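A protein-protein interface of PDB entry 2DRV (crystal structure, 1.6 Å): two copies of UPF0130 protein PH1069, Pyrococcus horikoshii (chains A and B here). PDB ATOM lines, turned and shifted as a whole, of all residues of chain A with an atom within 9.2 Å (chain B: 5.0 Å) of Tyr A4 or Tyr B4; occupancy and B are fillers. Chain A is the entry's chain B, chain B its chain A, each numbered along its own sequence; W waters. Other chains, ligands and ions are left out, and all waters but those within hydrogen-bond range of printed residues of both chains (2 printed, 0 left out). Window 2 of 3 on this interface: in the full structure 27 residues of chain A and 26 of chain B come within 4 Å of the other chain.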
ATOM      1  N   MET A   1      -9.325  22.127 -40.723  1.00  0.00           N
ATOM      2  CA  MET A   1      -9.297  22.554 -39.330  1.00  0.00           C
ATOM      3  C   MET A   1      -9.653  21.405 -38.382  1.00  0.00           C
ATOM      4  O   MET A   1     -10.756  20.878 -38.383  1.00  0.00           O
ATOM      5  CB  MET A   1     -10.311  23.689 -39.163  1.00  0.00           C
ATOM      6  CG  MET A   1     -10.130  24.453 -37.849  1.00  0.00           C
ATOM      7  SD  MET A   1     -11.071  25.985 -37.814  1.00  0.00           S
ATOM      8  CE  MET A   1     -12.653  25.294 -37.306  1.00  0.00           C
ATOM      9  N   LEU A   2      -8.649  20.986 -37.581  1.00  0.00           N
ATOM     10  CA  LEU A   2      -8.946  20.011 -36.545  1.00  0.00           C
ATOM     11  C   LEU A   2      -9.787  20.658 -35.454  1.00  0.00           C
ATOM     12  O   LEU A   2      -9.504  21.739 -34.953  1.00  0.00           O
ATOM     13  CB  LEU A   2      -7.636  19.487 -35.952  1.00  0.00           C
ATOM     14  CG  LEU A   2      -7.875  18.699 -34.662  1.00  0.00           C
ATOM     15  CD1 LEU A   2      -8.338  17.265 -34.929  1.00  0.00           C
ATOM     16  CD2 LEU A   2      -6.624  18.592 -33.791  1.00  0.00           C
ATOM     17  N   LEU A   3     -10.896  19.992 -35.137  1.00  0.00           N
ATOM     18  CA  LEU A   3     -11.771  20.567 -34.136  1.00  0.00           C
ATOM     19  C   LEU A   3     -11.506  19.953 -32.766  1.00  0.00           C
ATOM     20  O   LEU A   3     -11.809  18.795 -32.512  1.00  0.00           O
ATOM     21  CB  LEU A   3     -13.213  20.305 -34.554  1.00  0.00           C
ATOM     22  CG  LEU A   3     -13.681  21.248 -35.661  1.00  0.00           C
ATOM     23  CD1 LEU A   3     -15.182  21.129 -35.929  1.00  0.00           C
ATOM     24  CD2 LEU A   3     -13.418  22.721 -35.341  1.00  0.00           C
ATOM     25  N   TYR A   4     -10.885  20.635 -31.810  1.00  0.00           N
ATOM     26  CA  TYR A   4     -10.552  20.022 -30.535  1.00  0.00           C
ATOM     27  C   TYR A   4     -11.713  19.311 -29.861  1.00  0.00           C
ATOM     28  O   TYR A   4     -12.802  19.864 -29.724  1.00  0.00           O
ATOM     29  CB  TYR A   4      -9.994  21.068 -29.568  1.00  0.00           C
ATOM     30  CG  TYR A   4      -8.546  21.463 -29.778  1.00  0.00           C
ATOM     31  CD1 TYR A   4      -7.731  20.808 -30.704  1.00  0.00           C
ATOM     32  CD2 TYR A   4      -7.987  22.495 -29.031  1.00  0.00           C
ATOM     33  CE1 TYR A   4      -6.395  21.181 -30.871  1.00  0.00           C
ATOM     34  CE2 TYR A   4      -6.670  22.870 -29.186  1.00  0.00           C
ATOM     35  CZ  TYR A   4      -5.874  22.216 -30.105  1.00  0.00           C
ATOM     36  OH  TYR A   4      -4.570  22.616 -30.249  1.00  0.00           O
ATOM     37  N   MET A   5     -11.451  18.079 -29.439  1.00  0.00           N
ATOM     38  CA  MET A   5     -12.408  17.231 -28.736  1.00  0.00           C
ATOM     39  C   MET A   5     -13.559  16.673 -29.565  1.00  0.00           C
ATOM     40  O   MET A   5     -14.373  15.914 -29.046  1.00  0.00           O
ATOM     41  CB  MET A   5     -12.969  17.964 -27.512  1.00  0.00           C
ATOM     42  CG  MET A   5     -11.902  18.464 -26.557  1.00  0.00           C
ATOM     43  SD  MET A   5     -12.656  19.245 -24.964  1.00  0.00           S
ATOM     44  CE  MET A   5     -13.332  20.879 -25.734  1.00  0.00           C
ATOM     45  N   ARG A   6     -13.629  17.037 -30.842  1.00  0.00           N
ATOM     46  CA  ARG A   6     -14.693  16.525 -31.698  1.00  0.00           C
ATOM     47  C   ARG A   6     -14.657  14.996 -31.786  1.00  0.00           C
ATOM     48  O   ARG A   6     -15.702  14.356 -31.832  1.00  0.00           O
ATOM     49  CB  ARG A   6     -14.601  17.128 -33.105  1.00  0.00           C
ATOM     50  CG  ARG A   6     -15.549  18.295 -33.343  1.00  0.00           C
ATOM     51  CD  ARG A   6     -16.999  17.858 -33.137  1.00  0.00           C
ATOM     52  NE  ARG A   6     -17.941  18.964 -33.270  1.00  0.00           N
ATOM     53  CZ  ARG A   6     -18.270  19.538 -34.423  1.00  0.00           C
ATOM     54  NH1 ARG A   6     -17.736  19.110 -35.558  1.00  0.00           N
ATOM     55  NH2 ARG A   6     -19.134  20.542 -34.441  1.00  0.00           N
ATOM     56  N   PHE A   7     -13.466  14.400 -31.795  1.00  0.00           N
ATOM     57  CA  PHE A   7     -13.399  12.940 -31.881  1.00  0.00           C
ATOM     58  C   PHE A   7     -13.990  12.290 -30.632  1.00  0.00           C
ATOM     59  O   PHE A   7     -14.533  11.188 -30.688  1.00  0.00           O
ATOM     60  CB  PHE A   7     -11.953  12.470 -32.114  1.00  0.00           C
ATOM     61  CG  PHE A   7     -11.065  12.565 -30.907  1.00  0.00           C
ATOM     62  CD1 PHE A   7     -10.385  13.743 -30.622  1.00  0.00           C
ATOM     63  CD2 PHE A   7     -10.866  11.460 -30.082  1.00  0.00           C
ATOM     64  CE1 PHE A   7      -9.515  13.819 -29.534  1.00  0.00           C
ATOM     65  CE2 PHE A   7      -9.993  11.525 -28.990  1.00  0.00           C
ATOM     66  CZ  PHE A   7      -9.316  12.707 -28.719  1.00  0.00           C
ATOM     67  N   THR A   8     -13.893  12.987 -29.503  1.00  0.00           N
ATOM     68  CA  THR A   8     -14.435  12.491 -28.248  1.00  0.00           C
ATOM     69  C   THR A   8     -15.955  12.571 -28.319  1.00  0.00           C
ATOM     70  O   THR A   8     -16.662  11.660 -27.890  1.00  0.00           O
ATOM     71  CB  THR A   8     -13.936  13.342 -27.074  1.00  0.00           C
ATOM     72  OG1 THR A   8     -12.506  13.264 -27.015  1.00  0.00           O
ATOM     73  CG2 THR A   8     -14.533  12.850 -25.761  1.00  0.00           C
ATOM     74  N   GLU A   9     -16.445  13.674 -28.874  1.00  0.00           N
ATOM     75  CA  GLU A   9     -17.873  13.892 -29.040  1.00  0.00           C
ATOM     76  C   GLU A   9     -18.448  12.846 -29.994  1.00  0.00           C
ATOM     77  O   GLU A   9     -19.579  12.391 -29.830  1.00  0.00           O
ATOM     78  CB  GLU A   9     -18.114  15.295 -29.600  1.00  0.00           C
ATOM     79  CG  GLU A   9     -17.848  16.409 -28.592  1.00  0.00           C
ATOM     80  CD  GLU A   9     -17.404  17.708 -29.241  1.00  0.00           C
ATOM     81  OE1 GLU A   9     -17.808  17.975 -30.392  1.00  0.00           O
ATOM     82  OE2 GLU A   9     -16.659  18.470 -28.589  1.00  0.00           O
ATOM     83  N   ASN A  10     -17.650  12.462 -30.983  1.00  0.00           N
ATOM     84  CA  ASN A  10     -18.074  11.479 -31.978  1.00  0.00           C
ATOM     85  C   ASN A  10     -17.728  10.029 -31.638  1.00  0.00           C
ATOM     86  O   ASN A  10     -18.049   9.119 -32.404  1.00  0.00           O
ATOM     87  CB  ASN A  10     -17.453  11.813 -33.337  1.00  0.00           C
ATOM     88  CG  ASN A  10     -17.983  13.107 -33.924  1.00  0.00           C
ATOM     89  OD1 ASN A  10     -19.167  13.421 -33.795  1.00  0.00           O
ATOM     90  ND2 ASN A  10     -17.113  13.853 -34.594  1.00  0.00           N
ATOM     91  N   ALA A 112      -9.470   5.654 -29.830  1.00  0.00           N
ATOM     92  CA  ALA A 112      -9.503   5.963 -28.398  1.00  0.00           C
ATOM     93  C   ALA A 112     -10.450   7.135 -28.158  1.00  0.00           C
ATOM     94  O   ALA A 112     -10.544   8.035 -28.982  1.00  0.00           O
ATOM     95  CB  ALA A 112      -8.100   6.313 -27.900  1.00  0.00           C
ATOM     96  N   LYS A 113     -11.136   7.123 -27.017  1.00  0.00           N
ATOM     97  CA  LYS A 113     -12.097   8.173 -26.693  1.00  0.00           C
ATOM     98  C   LYS A 113     -11.474   9.521 -26.344  1.00  0.00           C
ATOM     99  O   LYS A 113     -12.054  10.570 -26.642  1.00  0.00           O
ATOM    100  CB  LYS A 113     -12.999   7.712 -25.544  1.00  0.00           C
ATOM    101  CG  LYS A 113     -14.161   8.645 -25.271  1.00  0.00           C
ATOM    102  CD  LYS A 113     -14.973   8.182 -24.078  1.00  0.00           C
ATOM    103  CE  LYS A 113     -16.187   9.073 -23.892  1.00  0.00           C
ATOM    104  NZ  LYS A 113     -15.802  10.508 -23.971  1.00  0.00           N
ATOM    105  N   THR A 114     -10.308   9.492 -25.707  1.00  0.00           N
ATOM    106  CA  THR A 114      -9.618  10.722 -25.320  1.00  0.00           C
ATOM    107  C   THR A 114      -8.131  10.593 -25.590  1.00  0.00           C
ATOM    108  O   THR A 114      -7.627   9.498 -25.844  1.00  0.00           O
ATOM    109  CB  THR A 114      -9.779  11.036 -23.810  1.00  0.00           C
ATOM    110  OG1 THR A 114      -9.084  10.057 -23.027  1.00  0.00           O
ATOM    111  CG2 THR A 114     -11.243  11.053 -23.418  1.00  0.00           C
ATOM    112  N   LEU A 115      -7.429  11.719 -25.528  1.00  0.00           N
ATOM    113  CA  LEU A 115      -5.992  11.716 -25.743  1.00  0.00           C
ATOM    114  C   LEU A 115      -5.320  10.896 -24.647  1.00  0.00           C
ATOM    115  O   LEU A 115      -4.364  10.165 -24.903  1.00  0.00           O
ATOM    116  CB  LEU A 115      -5.446  13.148 -25.720  1.00  0.00           C
ATOM    117  CG  LEU A 115      -3.928  13.268 -25.847  1.00  0.00           C
ATOM    118  CD1 LEU A 115      -3.487  12.752 -27.212  1.00  0.00           C
ATOM    119  CD2 LEU A 115      -3.516  14.728 -25.678  1.00  0.00           C
ATOM    120  N   GLU A 116      -5.827  11.026 -23.424  1.00  0.00           N
ATOM    121  CA  GLU A 116      -5.282  10.297 -22.287  1.00  0.00           C
ATOM    122  C   GLU A 116      -5.428   8.793 -22.487  1.00  0.00           C
ATOM    123  O   GLU A 116      -4.502   8.032 -22.211  1.00  0.00           O
ATOM    124  CB  GLU A 116      -5.990  10.714 -20.997  1.00  0.00           C
ATOM    125  CG  GLU A 116      -5.439  10.018 -19.761  1.00  0.00           C
ATOM    126  CD  GLU A 116      -6.199  10.376 -18.501  1.00  0.00           C
ATOM    127  OE1 GLU A 116      -6.395  11.583 -18.249  1.00  0.00           O
ATOM    128  OE2 GLU A 116      -6.596   9.450 -17.761  1.00  0.00           O
ATOM    129  N   ASP A 117      -6.599   8.368 -22.953  1.00  0.00           N
ATOM    130  CA  ASP A 117      -6.830   6.950 -23.192  1.00  0.00           C
ATOM    131  C   ASP A 117      -5.850   6.448 -24.252  1.00  0.00           C
ATOM    132  O   ASP A 117      -5.314   5.345 -24.140  1.00  0.00           O
ATOM    133  CB  ASP A 117      -8.265   6.705 -23.659  1.00  0.00           C
ATOM    134  CG  ASP A 117      -9.290   6.962 -22.569  1.00  0.00           C
ATOM    135  OD1 ASP A 117      -9.080   6.494 -21.431  1.00  0.00           O
ATOM    136  OD2 ASP A 117     -10.309   7.621 -22.859  1.00  0.00           O
ATOM    137  N   ALA A 118      -5.614   7.262 -25.275  1.00  0.00           N
ATOM    138  CA  ALA A 118      -4.693   6.887 -26.347  1.00  0.00           C
ATOM    139  C   ALA A 118      -3.280   6.680 -25.816  1.00  0.00           C
ATOM    140  O   ALA A 118      -2.628   5.686 -26.126  1.00  0.00           O
ATOM    141  CB  ALA A 118      -4.684   7.958 -27.430  1.00  0.00           C
ATOM    142  N   ILE A 138      -5.256  12.046 -35.692  1.00  0.00           N
ATOM    143  CA  ILE A 138      -6.278  12.693 -34.888  1.00  0.00           C
ATOM    144  C   ILE A 138      -7.088  13.531 -35.858  1.00  0.00           C
ATOM    145  O   ILE A 138      -6.562  14.457 -36.475  1.00  0.00           O
ATOM    146  CB  ILE A 138      -5.688  13.645 -33.827  1.00  0.00           C
ATOM    147  CG1 ILE A 138      -4.666  12.912 -32.955  1.00  0.00           C
ATOM    148  CG2 ILE A 138      -6.810  14.165 -32.933  1.00  0.00           C
ATOM    149  CD1 ILE A 138      -4.121  13.765 -31.811  1.00  0.00           C
ATOM    150  N   SER A 139      -8.362  13.192 -36.007  1.00  0.00           N
ATOM    151  CA  SER A 139      -9.247  13.931 -36.896  1.00  0.00           C
ATOM    152  C   SER A 139     -10.460  14.333 -36.077  1.00  0.00           C
ATOM    153  O   SER A 139     -10.457  14.209 -34.847  1.00  0.00           O
ATOM    154  CB  SER A 139      -9.697  13.052 -38.066  1.00  0.00           C
ATOM    155  OG  SER A 139     -10.577  12.030 -37.630  1.00  0.00           O
ATOM    156  N   ASN A 140     -11.491  14.826 -36.753  1.00  0.00           N
ATOM    157  CA  ASN A 140     -12.715  15.210 -36.063  1.00  0.00           C
ATOM    158  C   ASN A 140     -13.606  13.993 -35.873  1.00  0.00           C
ATOM    159  O   ASN A 140     -14.571  14.030 -35.116  1.00  0.00           O
ATOM    160  CB  ASN A 140     -13.463  16.288 -36.850  1.00  0.00           C
ATOM    161  CG  ASN A 140     -12.670  17.572 -36.962  1.00  0.00           C
ATOM    162  OD1 ASN A 140     -11.859  17.885 -36.092  1.00  0.00           O
ATOM    163  ND2 ASN A 140     -12.906  18.328 -38.026  1.00  0.00           N
ATOM    164  N   LEU A 143      -9.526   9.260 -33.157  1.00  0.00           N
ATOM    165  CA  LEU A 143      -8.103   9.318 -32.852  1.00  0.00           C
ATOM    166  C   LEU A 143      -7.652   7.866 -32.980  1.00  0.00           C
ATOM    167  O   LEU A 143      -8.161   6.984 -32.288  1.00  0.00           O
ATOM    168  CB  LEU A 143      -7.864   9.836 -31.427  1.00  0.00           C
ATOM    169  CG  LEU A 143      -6.394   9.987 -31.006  1.00  0.00           C
ATOM    170  CD1 LEU A 143      -6.293  10.911 -29.794  1.00  0.00           C
ATOM    171  CD2 LEU A 143      -5.797   8.630 -30.697  1.00  0.00           C
ATOM    172  N   LEU B   2      -1.952  15.882 -19.558  1.00  0.00           N
ATOM    173  CA  LEU B   2      -1.886  16.269 -20.991  1.00  0.00           C
ATOM    174  C   LEU B   2      -2.735  17.505 -21.244  1.00  0.00           C
ATOM    175  O   LEU B   2      -3.929  17.518 -20.954  1.00  0.00           O
ATOM    176  CB  LEU B   2      -2.388  15.121 -21.868  1.00  0.00           C
ATOM    177  CG  LEU B   2      -1.606  13.819 -21.725  1.00  0.00           C
ATOM    178  CD1 LEU B   2      -2.304  12.717 -22.509  1.00  0.00           C
ATOM    179  CD2 LEU B   2      -0.183  14.020 -22.224  1.00  0.00           C
ATOM    180  N   LEU B   3      -2.106  18.543 -21.777  1.00  0.00           N
ATOM    181  CA  LEU B   3      -2.799  19.787 -22.075  1.00  0.00           C
ATOM    182  C   LEU B   3      -2.681  20.080 -23.566  1.00  0.00           C
ATOM    183  O   LEU B   3      -1.588  20.103 -24.117  1.00  0.00           O
ATOM    184  CB  LEU B   3      -2.191  20.932 -21.254  1.00  0.00           C
ATOM    185  CG  LEU B   3      -2.417  20.874 -19.736  1.00  0.00           C
ATOM    186  CD1 LEU B   3      -1.434  21.797 -19.024  1.00  0.00           C
ATOM    187  CD2 LEU B   3      -3.859  21.266 -19.412  1.00  0.00           C
ATOM    188  N   TYR B   4      -3.816  20.291 -24.222  1.00  0.00           N
ATOM    189  CA  TYR B   4      -3.825  20.582 -25.647  1.00  0.00           C
ATOM    190  C   TYR B   4      -2.984  21.804 -26.013  1.00  0.00           C
ATOM    191  O   TYR B   4      -2.302  21.806 -27.037  1.00  0.00           O
ATOM    192  CB  TYR B   4      -5.261  20.803 -26.124  1.00  0.00           C
ATOM    193  CG  TYR B   4      -6.042  19.549 -26.447  1.00  0.00           C
ATOM    194  CD1 TYR B   4      -5.892  18.385 -25.697  1.00  0.00           C
ATOM    195  CD2 TYR B   4      -6.980  19.557 -27.478  1.00  0.00           C
ATOM    196  CE1 TYR B   4      -6.671  17.251 -25.968  1.00  0.00           C
ATOM    197  CE2 TYR B   4      -7.758  18.442 -27.754  1.00  0.00           C
ATOM    198  CZ  TYR B   4      -7.602  17.296 -27.000  1.00  0.00           C
ATOM    199  OH  TYR B   4      -8.391  16.204 -27.290  1.00  0.00           O
ATOM    200  N   MET B   5      -3.026  22.846 -25.185  1.00  0.00           N
ATOM    201  CA  MET B   5      -2.268  24.058 -25.486  1.00  0.00           C
ATOM    202  C   MET B   5      -0.838  24.043 -24.962  1.00  0.00           C
ATOM    203  O   MET B   5      -0.098  25.017 -25.123  1.00  0.00           O
ATOM    204  CB  MET B   5      -3.010  25.290 -24.960  1.00  0.00           C
ATOM    205  CG  MET B   5      -4.283  25.584 -25.736  1.00  0.00           C
ATOM    206  SD  MET B   5      -5.091  27.245 -25.181  1.00  0.00           S
ATOM    207  CE  MET B   5      -6.025  26.591 -23.660  1.00  0.00           C
ATOM    208  N   ARG B   6      -0.460  22.928 -24.350  1.00  0.00           N
ATOM    209  CA  ARG B   6       0.877  22.731 -23.806  1.00  0.00           C
ATOM    210  C   ARG B   6       1.286  21.313 -24.196  1.00  0.00           C
ATOM    211  O   ARG B   6       1.594  20.476 -23.347  1.00  0.00           O
ATOM    212  CB  ARG B   6       0.858  22.876 -22.281  1.00  0.00           C
ATOM    213  CG  ARG B   6       0.446  24.256 -21.781  1.00  0.00           C
ATOM    214  CD  ARG B   6       1.545  25.290 -21.995  1.00  0.00           C
ATOM    215  NE  ARG B   6       1.207  26.567 -21.373  1.00  0.00           N
ATOM    216  CZ  ARG B   6       2.020  27.619 -21.324  1.00  0.00           C
ATOM    217  NH1 ARG B   6       3.231  27.555 -21.861  1.00  0.00           N
ATOM    218  NH2 ARG B   6       1.618  28.739 -20.736  1.00  0.00           N
ATOM    219  N   PHE B   7       1.271  21.058 -25.501  1.00  0.00           N
ATOM    220  CA  PHE B   7       1.607  19.749 -26.047  1.00  0.00           C
ATOM    221  C   PHE B   7       2.984  19.273 -25.592  1.00  0.00           C
ATOM    222  O   PHE B   7       3.125  18.162 -25.086  1.00  0.00           O
ATOM    223  CB  PHE B   7       1.510  19.807 -27.573  1.00  0.00           C
ATOM    224  CG  PHE B   7       1.898  18.533 -28.255  1.00  0.00           C
ATOM    225  CD1 PHE B   7       0.962  17.523 -28.457  1.00  0.00           C
ATOM    226  CD2 PHE B   7       3.201  18.342 -28.696  1.00  0.00           C
ATOM    227  CE1 PHE B   7       1.326  16.336 -29.093  1.00  0.00           C
ATOM    228  CE2 PHE B   7       3.570  17.163 -29.332  1.00  0.00           C
ATOM    229  CZ  PHE B   7       2.629  16.163 -29.528  1.00  0.00           C
ATOM    230  N   LYS B 113       4.189  23.359 -29.681  1.00  0.00           N
ATOM    231  CA  LYS B 113       3.487  24.085 -28.631  1.00  0.00           C
ATOM    232  C   LYS B 113       2.114  23.520 -28.293  1.00  0.00           C
ATOM    233  O   LYS B 113       1.804  23.327 -27.117  1.00  0.00           O
ATOM    234  CB  LYS B 113       3.341  25.560 -29.002  1.00  0.00           C
ATOM    235  CG  LYS B 113       4.608  26.372 -28.809  1.00  0.00           C
ATOM    236  CD  LYS B 113       4.311  27.853 -28.916  1.00  0.00           C
ATOM    237  CE  LYS B 113       5.552  28.681 -28.658  1.00  0.00           C
ATOM    238  NZ  LYS B 113       5.208  30.122 -28.489  1.00  0.00           N
ATOM    239  N   THR B 114       1.298  23.259 -29.313  1.00  0.00           N
ATOM    240  CA  THR B 114      -0.054  22.746 -29.094  1.00  0.00           C
ATOM    241  C   THR B 114      -0.358  21.488 -29.892  1.00  0.00           C
ATOM    242  O   THR B 114       0.379  21.127 -30.814  1.00  0.00           O
ATOM    243  CB  THR B 114      -1.119  23.783 -29.489  1.00  0.00           C
ATOM    244  OG1 THR B 114      -1.176  23.892 -30.916  1.00  0.00           O
ATOM    245  CG2 THR B 114      -0.776  25.145 -28.901  1.00  0.00           C
ATOM    246  N   LEU B 115      -1.461  20.841 -29.540  1.00  0.00           N
ATOM    247  CA  LEU B 115      -1.867  19.627 -30.233  1.00  0.00           C
ATOM    248  C   LEU B 115      -2.155  19.954 -31.696  1.00  0.00           C
ATOM    249  O   LEU B 115      -1.801  19.182 -32.593  1.00  0.00           O
ATOM    250  CB  LEU B 115      -3.108  19.020 -29.564  1.00  0.00           C
ATOM    251  CG  LEU B 115      -3.526  17.648 -30.111  1.00  0.00           C
ATOM    252  CD1 LEU B 115      -2.396  16.642 -29.889  1.00  0.00           C
ATOM    253  CD2 LEU B 115      -4.802  17.183 -29.427  1.00  0.00           C
ATOM    254  N   GLU B 116      -2.794  21.098 -31.943  1.00  0.00           N
ATOM    255  CA  GLU B 116      -3.091  21.506 -33.312  1.00  0.00           C
ATOM    256  C   GLU B 116      -1.791  21.614 -34.106  1.00  0.00           C
ATOM    257  O   GLU B 116      -1.726  21.198 -35.261  1.00  0.00           O
ATOM    258  CB  GLU B 116      -3.824  22.854 -33.344  1.00  0.00           C
ATOM    259  CG  GLU B 116      -3.838  23.491 -34.728  1.00  0.00           C
ATOM    260  CD  GLU B 116      -4.513  24.850 -34.758  1.00  0.00           C
ATOM    261  OE1 GLU B 116      -4.464  25.566 -33.737  1.00  0.00           O
ATOM    262  OE2 GLU B 116      -5.076  25.207 -35.813  1.00  0.00           O
HETATM  263  O   HOH W   1      -7.339  23.888 -34.504  1.00  0.00           O
HETATM  264  O   HOH W   2      -8.724  14.262 -25.301  1.00  0.00           O
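Water W2 lies within hydrogen-bond range of the side-chain hydroxyl (OH) of Tyr B4 (2.8 Å) and the backbone NH (N) of Leu A115 (2.9 Å). Water W1 lies within hydrogen-bond range of OE2 of Glu B116 and O of Leu A2.
Leu A2 touches none of the printed residues of chain B. Of the printed residues of chain B, Tyr A4 touches Tyr B4, Thr B114, Leu B115 and Glu B116. Lys A113 touches none of the printed residues of chain B. Of the printed residues of chain B, Leu A115 touches Leu B2 (3.8 Å). Of the printed residues of chain B, Ile A138 touches Leu B115. Printed residues of chain A within 4 Å of Leu B2: Leu A115 (3.8 Å) and Glu A116 (3.8 Å). Tyr B4 touches two residues of chain A.
The backbone NH (N) of Glu B116 sits at hydrogen-bond distance from the side-chain hydroxyl (OH) of Tyr A4 (2.9 Å).
Tyr A4 touches its own counterpart, Tyr B4. Tyr A4 touches Thr B114, but with the chains exchanged Thr A114 does not touch Tyr B4 (5.9 Å). Tyr A4 touches Leu B115, but with the chains exchanged Leu A115 does not touch Tyr B4 (4.1 Å). Tyr A4 touches Glu B116, but with the chains exchanged Glu A116 does not touch Tyr B4 (6.8 Å).
Hydrophobic or aromatic side chains of chain B that line the printed part of chain A: Leu B2, Tyr B4 and Leu B115. Of the 21 printed residues of chain A, 5 touch a printed residue of chain B. Hydrophobic or aromatic side chains of chain A that line the printed part of chain B: Tyr A4, Phe A7, Leu A115 and Ile A138. Among the printed residues, 8 pairs touch across the chains. Among the printed residues, no Asp or Glu carboxylate lies within 4 Å of a Lys or Arg side-chain nitrogen of the other chain.
Tyr A4 touches Tyr B4 (CG to CD2, 3.4 Å). Tyr A4 touches Thr B114 (OH to OG1, 3.7 Å). Tyr A4 touches Leu B115 (OH to N, 3.6 Å). Phe A7 touches Tyr B4. Leu A115 touches Leu B2 (CG to CD1, 3.8 Å). Leu B2 touches Glu A116 (CD1 to CA, 3.8 Å). Leu B115 touches Ile A138.
The backbone carbonyl oxygen (O) of Tyr B4 sits at hydrogen-bond distance from the backbone NH (N) of Leu B115. N of Glu B116 sits close to OG1 of Thr B114 (3.4 Å). The side-chain hydroxyl of Thr A114 lies close to the backbone NH of Glu A116 (3.4 Å).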
